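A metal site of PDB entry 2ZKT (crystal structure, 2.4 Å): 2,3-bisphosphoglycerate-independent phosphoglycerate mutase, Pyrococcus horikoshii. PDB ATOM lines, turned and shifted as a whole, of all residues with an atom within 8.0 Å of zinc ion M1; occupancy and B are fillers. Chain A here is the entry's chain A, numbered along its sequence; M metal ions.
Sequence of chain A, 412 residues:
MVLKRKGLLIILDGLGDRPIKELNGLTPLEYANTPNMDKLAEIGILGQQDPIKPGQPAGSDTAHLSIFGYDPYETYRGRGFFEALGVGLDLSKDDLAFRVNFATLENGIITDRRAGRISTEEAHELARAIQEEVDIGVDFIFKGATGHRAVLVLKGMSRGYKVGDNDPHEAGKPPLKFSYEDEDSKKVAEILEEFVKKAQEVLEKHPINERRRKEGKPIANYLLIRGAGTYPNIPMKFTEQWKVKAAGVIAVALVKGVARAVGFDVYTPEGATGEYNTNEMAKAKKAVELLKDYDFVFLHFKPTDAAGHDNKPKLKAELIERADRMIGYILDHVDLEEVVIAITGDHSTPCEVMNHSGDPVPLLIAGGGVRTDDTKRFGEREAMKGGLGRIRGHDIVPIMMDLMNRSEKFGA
The nearest printed residue that does not touch zinc ion M1 is His 356 (4.3 Å).
The backbone carbonyl oxygen (O) of Ser 60 is in hydrogen-bond range of a ring nitrogen (ND1) of His 64 (2.7 Å). The backbone NH (N) of Gly 14 lies within hydrogen-bond range of the side-chain carboxylate (OD1) of Asp 346, at 3.3 Å. The backbone carbonyl oxygen (O) of Asp 13 sits at hydrogen-bond distance from the backbone NH (N) of Asp 305, at 3.0 Å. The side-chain carboxylate (OD2) of Asp 13 is in hydrogen-bond range of a ring nitrogen (NE2) of His 300. The backbone NH (N) of Asp 13 sits at hydrogen-bond distance from the backbone carbonyl oxygen (O) of Phe 301 (2.9 Å). A ring nitrogen (ND1) of His 347 lies close to the side-chain hydroxyl of Thr 349, 3.2 Å away.
Zinc ion M1 is bound by OG of Ser 60, OD2 of Asp 346, OD1 of Asp 13 and NE2 of His 347. Zinc ion M1 has four donor atoms within binding distance. Slightly farther from zinc ion M1 lies the side-chain carboxylate (OD2) of Asp 13 (2.7 Å).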
ATOM      1  N   ILE A  11      11.738  -7.546  14.152  1.00  0.00           N
ATOM      2  CA  ILE A  11      12.524  -8.242  13.160  1.00  0.00           C
ATOM      3  C   ILE A  11      12.025  -7.933  11.751  1.00  0.00           C
ATOM      4  O   ILE A  11      10.859  -8.182  11.416  1.00  0.00           O
ATOM      5  CB  ILE A  11      12.491  -9.776  13.375  1.00  0.00           C
ATOM      6  CG1 ILE A  11      13.267 -10.128  14.655  1.00  0.00           C
ATOM      7  CG2 ILE A  11      13.096 -10.489  12.183  1.00  0.00           C
ATOM      8  CD1 ILE A  11      14.742  -9.748  14.605  1.00  0.00           C
ATOM      9  N   LEU A  12      12.912  -7.378  10.934  1.00  0.00           N
ATOM     10  CA  LEU A  12      12.614  -7.074   9.545  1.00  0.00           C
ATOM     11  C   LEU A  12      13.347  -8.183   8.805  1.00  0.00           C
ATOM     12  O   LEU A  12      14.570  -8.122   8.611  1.00  0.00           O
ATOM     13  CB  LEU A  12      13.166  -5.694   9.156  1.00  0.00           C
ATOM     14  CG  LEU A  12      12.339  -4.462   9.561  1.00  0.00           C
ATOM     15  CD1 LEU A  12      11.779  -4.600  10.971  1.00  0.00           C
ATOM     16  CD2 LEU A  12      13.225  -3.236   9.448  1.00  0.00           C
ATOM     17  N   ASP A  13      12.605  -9.222   8.415  1.00  0.00           N
ATOM     18  CA  ASP A  13      13.182 -10.375   7.723  1.00  0.00           C
ATOM     19  C   ASP A  13      14.108  -9.961   6.571  1.00  0.00           C
ATOM     20  O   ASP A  13      13.769  -9.101   5.762  1.00  0.00           O
ATOM     21  CB  ASP A  13      12.033 -11.269   7.216  1.00  0.00           C
ATOM     22  CG  ASP A  13      12.389 -12.751   7.274  1.00  0.00           C
ATOM     23  OD1 ASP A  13      13.197 -13.201   6.420  1.00  0.00           O
ATOM     24  OD2 ASP A  13      11.868 -13.467   8.172  1.00  0.00           O
ATOM     25  N   GLY A  14      15.293 -10.584   6.528  1.00  0.00           N
ATOM     26  CA  GLY A  14      16.267 -10.293   5.472  1.00  0.00           C
ATOM     27  C   GLY A  14      16.822  -8.859   5.349  1.00  0.00           C
ATOM     28  O   GLY A  14      17.399  -8.514   4.306  1.00  0.00           O
ATOM     29  N   LEU A  15      16.639  -8.053   6.393  1.00  0.00           N
ATOM     30  CA  LEU A  15      17.108  -6.656   6.406  1.00  0.00           C
ATOM     31  C   LEU A  15      18.495  -6.415   5.762  1.00  0.00           C
ATOM     32  O   LEU A  15      18.651  -5.538   4.899  1.00  0.00           O
ATOM     33  CB  LEU A  15      17.146  -6.126   7.845  1.00  0.00           C
ATOM     34  CG  LEU A  15      17.423  -4.628   8.031  1.00  0.00           C
ATOM     35  CD1 LEU A  15      16.427  -3.799   7.212  1.00  0.00           C
ATOM     36  CD2 LEU A  15      17.312  -4.276   9.524  1.00  0.00           C
ATOM     37  N   ALA A  58      21.828 -18.500   7.575  1.00  0.00           N
ATOM     38  CA  ALA A  58      20.854 -19.225   8.389  1.00  0.00           C
ATOM     39  C   ALA A  58      19.452 -19.134   7.807  1.00  0.00           C
ATOM     40  O   ALA A  58      19.049 -18.081   7.288  1.00  0.00           O
ATOM     41  CB  ALA A  58      20.853 -18.684   9.816  1.00  0.00           C
ATOM     42  N   GLY A  59      18.700 -20.235   7.892  1.00  0.00           N
ATOM     43  CA  GLY A  59      17.329 -20.224   7.404  1.00  0.00           C
ATOM     44  C   GLY A  59      16.489 -19.371   8.342  1.00  0.00           C
ATOM     45  O   GLY A  59      16.921 -19.055   9.461  1.00  0.00           O
ATOM     46  N   SER A  60      15.285 -18.997   7.905  1.00  0.00           N
ATOM     47  CA  SER A  60      14.414 -18.159   8.743  1.00  0.00           C
ATOM     48  C   SER A  60      14.106 -18.806  10.106  1.00  0.00           C
ATOM     49  O   SER A  60      13.972 -18.118  11.120  1.00  0.00           O
ATOM     50  CB  SER A  60      13.114 -17.865   7.988  1.00  0.00           C
ATOM     51  OG  SER A  60      12.614 -16.583   8.352  1.00  0.00           O
ATOM     52  N   ASP A  61      13.985 -20.134  10.130  1.00  0.00           N
ATOM     53  CA  ASP A  61      13.682 -20.837  11.372  1.00  0.00           C
ATOM     54  C   ASP A  61      14.885 -20.970  12.324  1.00  0.00           C
ATOM     55  O   ASP A  61      14.751 -20.682  13.513  1.00  0.00           O
ATOM     56  CB  ASP A  61      13.077 -22.217  11.077  1.00  0.00           C
ATOM     57  CG  ASP A  61      13.921 -23.028  10.106  1.00  0.00           C
ATOM     58  OD1 ASP A  61      14.990 -22.523   9.653  1.00  0.00           O
ATOM     59  OD2 ASP A  61      13.519 -24.177   9.814  1.00  0.00           O
ATOM     60  N   THR A  62      16.055 -21.392  11.809  1.00  0.00           N
ATOM     61  CA  THR A  62      17.241 -21.507  12.673  1.00  0.00           C
ATOM     62  C   THR A  62      17.664 -20.115  13.166  1.00  0.00           C
ATOM     63  O   THR A  62      18.071 -19.954  14.319  1.00  0.00           O
ATOM     64  CB  THR A  62      18.454 -22.116  11.919  1.00  0.00           C
ATOM     65  OG1 THR A  62      18.588 -21.503  10.631  1.00  0.00           O
ATOM     66  CG2 THR A  62      18.286 -23.640  11.749  1.00  0.00           C
ATOM     67  N   ALA A  63      17.551 -19.106  12.301  1.00  0.00           N
ATOM     68  CA  ALA A  63      17.933 -17.742  12.679  1.00  0.00           C
ATOM     69  C   ALA A  63      17.075 -17.251  13.844  1.00  0.00           C
ATOM     70  O   ALA A  63      17.583 -16.600  14.773  1.00  0.00           O
ATOM     71  CB  ALA A  63      17.796 -16.802  11.491  1.00  0.00           C
ATOM     72  N   HIS A  64      15.780 -17.556  13.818  1.00  0.00           N
ATOM     73  CA  HIS A  64      14.888 -17.108  14.892  1.00  0.00           C
ATOM     74  C   HIS A  64      15.108 -17.915  16.176  1.00  0.00           C
ATOM     75  O   HIS A  64      14.841 -17.447  17.285  1.00  0.00           O
ATOM     76  CB  HIS A  64      13.418 -17.191  14.443  1.00  0.00           C
ATOM     77  CG  HIS A  64      13.005 -15.953  13.654  1.00  0.00           C
ATOM     78  ND1 HIS A  64      13.201 -15.830  12.317  1.00  0.00           N
ATOM     79  CD2 HIS A  64      12.361 -14.795  14.118  1.00  0.00           C
ATOM     80  CE1 HIS A  64      12.691 -14.617  11.994  1.00  0.00           C
ATOM     81  NE2 HIS A  64      12.181 -13.973  13.048  1.00  0.00           N
ATOM     82  N   VAL A 252       3.709 -14.902   9.034  1.00  0.00           N
ATOM     83  CA  VAL A 252       4.284 -16.069   8.366  1.00  0.00           C
ATOM     84  C   VAL A 252       4.230 -17.342   9.235  1.00  0.00           C
ATOM     85  O   VAL A 252       4.690 -17.345  10.381  1.00  0.00           O
ATOM     86  CB  VAL A 252       5.740 -15.808   7.965  1.00  0.00           C
ATOM     87  CG1 VAL A 252       6.277 -16.967   7.129  1.00  0.00           C
ATOM     88  CG2 VAL A 252       5.815 -14.513   7.182  1.00  0.00           C
ATOM     89  N   LEU A 254       5.908 -20.194   9.241  1.00  0.00           N
ATOM     90  CA  LEU A 254       7.195 -20.650   9.752  1.00  0.00           C
ATOM     91  C   LEU A 254       7.662 -19.957  11.034  1.00  0.00           C
ATOM     92  O   LEU A 254       8.069 -20.624  11.994  1.00  0.00           O
ATOM     93  CB  LEU A 254       8.276 -20.492   8.670  1.00  0.00           C
ATOM     94  CG  LEU A 254       9.654 -21.056   9.054  1.00  0.00           C
ATOM     95  CD1 LEU A 254       9.484 -22.399   9.779  1.00  0.00           C
ATOM     96  CD2 LEU A 254      10.506 -21.205   7.802  1.00  0.00           C
ATOM     97  N   VAL A 255       7.612 -18.624  11.075  1.00  0.00           N
ATOM     98  CA  VAL A 255       8.054 -17.896  12.254  1.00  0.00           C
ATOM     99  C   VAL A 255       7.053 -18.047  13.385  1.00  0.00           C
ATOM    100  O   VAL A 255       7.419 -17.986  14.577  1.00  0.00           O
ATOM    101  CB  VAL A 255       8.287 -16.375  11.955  1.00  0.00           C
ATOM    102  CG1 VAL A 255       8.658 -15.642  13.270  1.00  0.00           C
ATOM    103  CG2 VAL A 255       9.420 -16.200  10.951  1.00  0.00           C
ATOM    104  N   HIS A 300       7.264  -9.327  13.934  1.00  0.00           N
ATOM    105  CA  HIS A 300       7.924  -9.783  12.710  1.00  0.00           C
ATOM    106  C   HIS A 300       7.325  -9.166  11.435  1.00  0.00           C
ATOM    107  O   HIS A 300       6.107  -8.988  11.333  1.00  0.00           O
ATOM    108  CB  HIS A 300       7.864 -11.318  12.656  1.00  0.00           C
ATOM    109  CG  HIS A 300       8.491 -11.917  11.432  1.00  0.00           C
ATOM    110  ND1 HIS A 300       7.779 -12.117  10.254  1.00  0.00           N
ATOM    111  CD2 HIS A 300       9.744 -12.382  11.198  1.00  0.00           C
ATOM    112  CE1 HIS A 300       8.578 -12.672   9.357  1.00  0.00           C
ATOM    113  NE2 HIS A 300       9.771 -12.846   9.904  1.00  0.00           N
ATOM    114  N   PHE A 301       8.201  -8.838  10.474  1.00  0.00           N
ATOM    115  CA  PHE A 301       7.811  -8.234   9.189  1.00  0.00           C
ATOM    116  C   PHE A 301       8.518  -9.018   8.077  1.00  0.00           C
ATOM    117  O   PHE A 301       9.745  -8.927   7.916  1.00  0.00           O
ATOM    118  CB  PHE A 301       8.238  -6.760   9.160  1.00  0.00           C
ATOM    119  CG  PHE A 301       7.764  -5.980   7.951  1.00  0.00           C
ATOM    120  CD1 PHE A 301       6.413  -5.634   7.804  1.00  0.00           C
ATOM    121  CD2 PHE A 301       8.669  -5.558   6.963  1.00  0.00           C
ATOM    122  CE1 PHE A 301       5.966  -4.875   6.715  1.00  0.00           C
ATOM    123  CE2 PHE A 301       8.233  -4.793   5.861  1.00  0.00           C
ATOM    124  CZ  PHE A 301       6.882  -4.451   5.737  1.00  0.00           C
ATOM    125  N   LYS A 302       7.747  -9.785   7.310  1.00  0.00           N
ATOM    126  CA  LYS A 302       8.284 -10.660   6.259  1.00  0.00           C
ATOM    127  C   LYS A 302       8.737 -10.075   4.911  1.00  0.00           C
ATOM    128  O   LYS A 302       9.864 -10.315   4.470  1.00  0.00           O
ATOM    129  CB  LYS A 302       7.281 -11.793   5.993  1.00  0.00           C
ATOM    130  CG  LYS A 302       7.832 -12.923   5.118  1.00  0.00           C
ATOM    131  CD  LYS A 302       9.038 -13.568   5.777  1.00  0.00           C
ATOM    132  CE  LYS A 302       9.634 -14.641   4.895  1.00  0.00           C
ATOM    133  NZ  LYS A 302       9.849 -14.124   3.519  1.00  0.00           N
ATOM    134  N   ASP A 305      12.268  -9.500   3.158  1.00  0.00           N
ATOM    135  CA  ASP A 305      12.990 -10.688   2.691  1.00  0.00           C
ATOM    136  C   ASP A 305      12.597 -11.150   1.290  1.00  0.00           C
ATOM    137  O   ASP A 305      13.454 -11.602   0.519  1.00  0.00           O
ATOM    138  CB  ASP A 305      12.787 -11.834   3.694  1.00  0.00           C
ATOM    139  CG  ASP A 305      13.488 -13.121   3.275  1.00  0.00           C
ATOM    140  OD1 ASP A 305      14.729 -13.095   3.038  1.00  0.00           O
ATOM    141  OD2 ASP A 305      12.804 -14.160   3.196  1.00  0.00           O
ATOM    142  N   HIS A 309      14.995 -11.846  -2.214  1.00  0.00           N
ATOM    143  CA  HIS A 309      15.034 -13.064  -3.035  1.00  0.00           C
ATOM    144  C   HIS A 309      14.875 -12.782  -4.525  1.00  0.00           C
ATOM    145  O   HIS A 309      15.555 -13.411  -5.357  1.00  0.00           O
ATOM    146  CB  HIS A 309      13.928 -14.039  -2.595  1.00  0.00           C
ATOM    147  CG  HIS A 309      14.270 -14.830  -1.359  1.00  0.00           C
ATOM    148  ND1 HIS A 309      15.204 -15.853  -1.357  1.00  0.00           N
ATOM    149  CD2 HIS A 309      13.793 -14.756  -0.093  1.00  0.00           C
ATOM    150  CE1 HIS A 309      15.303 -16.365  -0.144  1.00  0.00           C
ATOM    151  NE2 HIS A 309      14.454 -15.721   0.645  1.00  0.00           N
ATOM    152  N   GLY A 345      17.435  -7.606  11.635  1.00  0.00           N
ATOM    153  CA  GLY A 345      16.919  -8.734  10.861  1.00  0.00           C
ATOM    154  C   GLY A 345      17.364 -10.075  11.450  1.00  0.00           C
ATOM    155  O   GLY A 345      18.202 -10.147  12.339  1.00  0.00           O
ATOM    156  N   ASP A 346      16.729 -11.163  10.958  1.00  0.00           N
ATOM    157  CA  ASP A 346      17.167 -12.495  11.388  1.00  0.00           C
ATOM    158  C   ASP A 346      18.330 -13.015  10.527  1.00  0.00           C
ATOM    159  O   ASP A 346      18.973 -14.005  10.836  1.00  0.00           O
ATOM    160  CB  ASP A 346      15.968 -13.450  11.315  1.00  0.00           C
ATOM    161  CG  ASP A 346      15.363 -13.411   9.912  1.00  0.00           C
ATOM    162  OD1 ASP A 346      15.375 -12.331   9.306  1.00  0.00           O
ATOM    163  OD2 ASP A 346      14.903 -14.450   9.434  1.00  0.00           O
ATOM    164  N   HIS A 347      18.550 -12.328   9.383  1.00  0.00           N
ATOM    165  CA  HIS A 347      19.701 -12.659   8.552  1.00  0.00           C
ATOM    166  C   HIS A 347      19.839 -11.685   7.361  1.00  0.00           C
ATOM    167  O   HIS A 347      19.036 -10.783   7.162  1.00  0.00           O
ATOM    168  CB  HIS A 347      19.534 -14.098   8.026  1.00  0.00           C
ATOM    169  CG  HIS A 347      18.212 -14.225   7.327  1.00  0.00           C
ATOM    170  ND1 HIS A 347      17.948 -13.665   6.114  1.00  0.00           N
ATOM    171  CD2 HIS A 347      17.074 -14.931   7.744  1.00  0.00           C
ATOM    172  CE1 HIS A 347      16.690 -14.024   5.801  1.00  0.00           C
ATOM    173  NE2 HIS A 347      16.134 -14.780   6.762  1.00  0.00           N
ATOM    174  N   SER A 348      20.877 -11.838   6.533  1.00  0.00           N
ATOM    175  CA  SER A 348      21.036 -10.960   5.378  1.00  0.00           C
ATOM    176  C   SER A 348      20.533 -11.703   4.163  1.00  0.00           C
ATOM    177  O   SER A 348      20.767 -12.906   4.020  1.00  0.00           O
ATOM    178  CB  SER A 348      22.511 -10.598   5.156  1.00  0.00           C
ATOM    179  OG  SER A 348      22.962  -9.693   6.150  1.00  0.00           O
ATOM    180  N   THR A 349      19.808 -10.987   3.298  1.00  0.00           N
ATOM    181  CA  THR A 349      19.293 -11.540   2.050  1.00  0.00           C
ATOM    182  C   THR A 349      19.639 -10.479   1.017  1.00  0.00           C
ATOM    183  O   THR A 349      18.801  -9.645   0.641  1.00  0.00           O
ATOM    184  CB  THR A 349      17.767 -11.732   2.080  1.00  0.00           C
ATOM    185  OG1 THR A 349      17.417 -12.628   3.139  1.00  0.00           O
ATOM    186  CG2 THR A 349      17.280 -12.322   0.748  1.00  0.00           C
ATOM    187  N   HIS A 356      19.746 -16.106   1.252  1.00  0.00           N
ATOM    188  CA  HIS A 356      20.363 -15.735   2.519  1.00  0.00           C
ATOM    189  C   HIS A 356      21.886 -15.788   2.434  1.00  0.00           C
ATOM    190  O   HIS A 356      22.462 -16.728   1.868  1.00  0.00           O
ATOM    191  CB  HIS A 356      19.867 -16.674   3.634  1.00  0.00           C
ATOM    192  CG  HIS A 356      18.376 -16.697   3.792  1.00  0.00           C
ATOM    193  ND1 HIS A 356      17.743 -17.413   4.795  1.00  0.00           N
ATOM    194  CD2 HIS A 356      17.387 -16.099   3.080  1.00  0.00           C
ATOM    195  CE1 HIS A 356      16.433 -17.258   4.691  1.00  0.00           C
ATOM    196  NE2 HIS A 356      16.191 -16.451   3.658  1.00  0.00           N
HETATM  197 ZN    ZN M   1      13.935 -15.097   7.472  1.00  0.00          ZN
HETATM  198 ZN    ZN M   2      14.003 -15.984   2.941  1.00  0.00          ZN
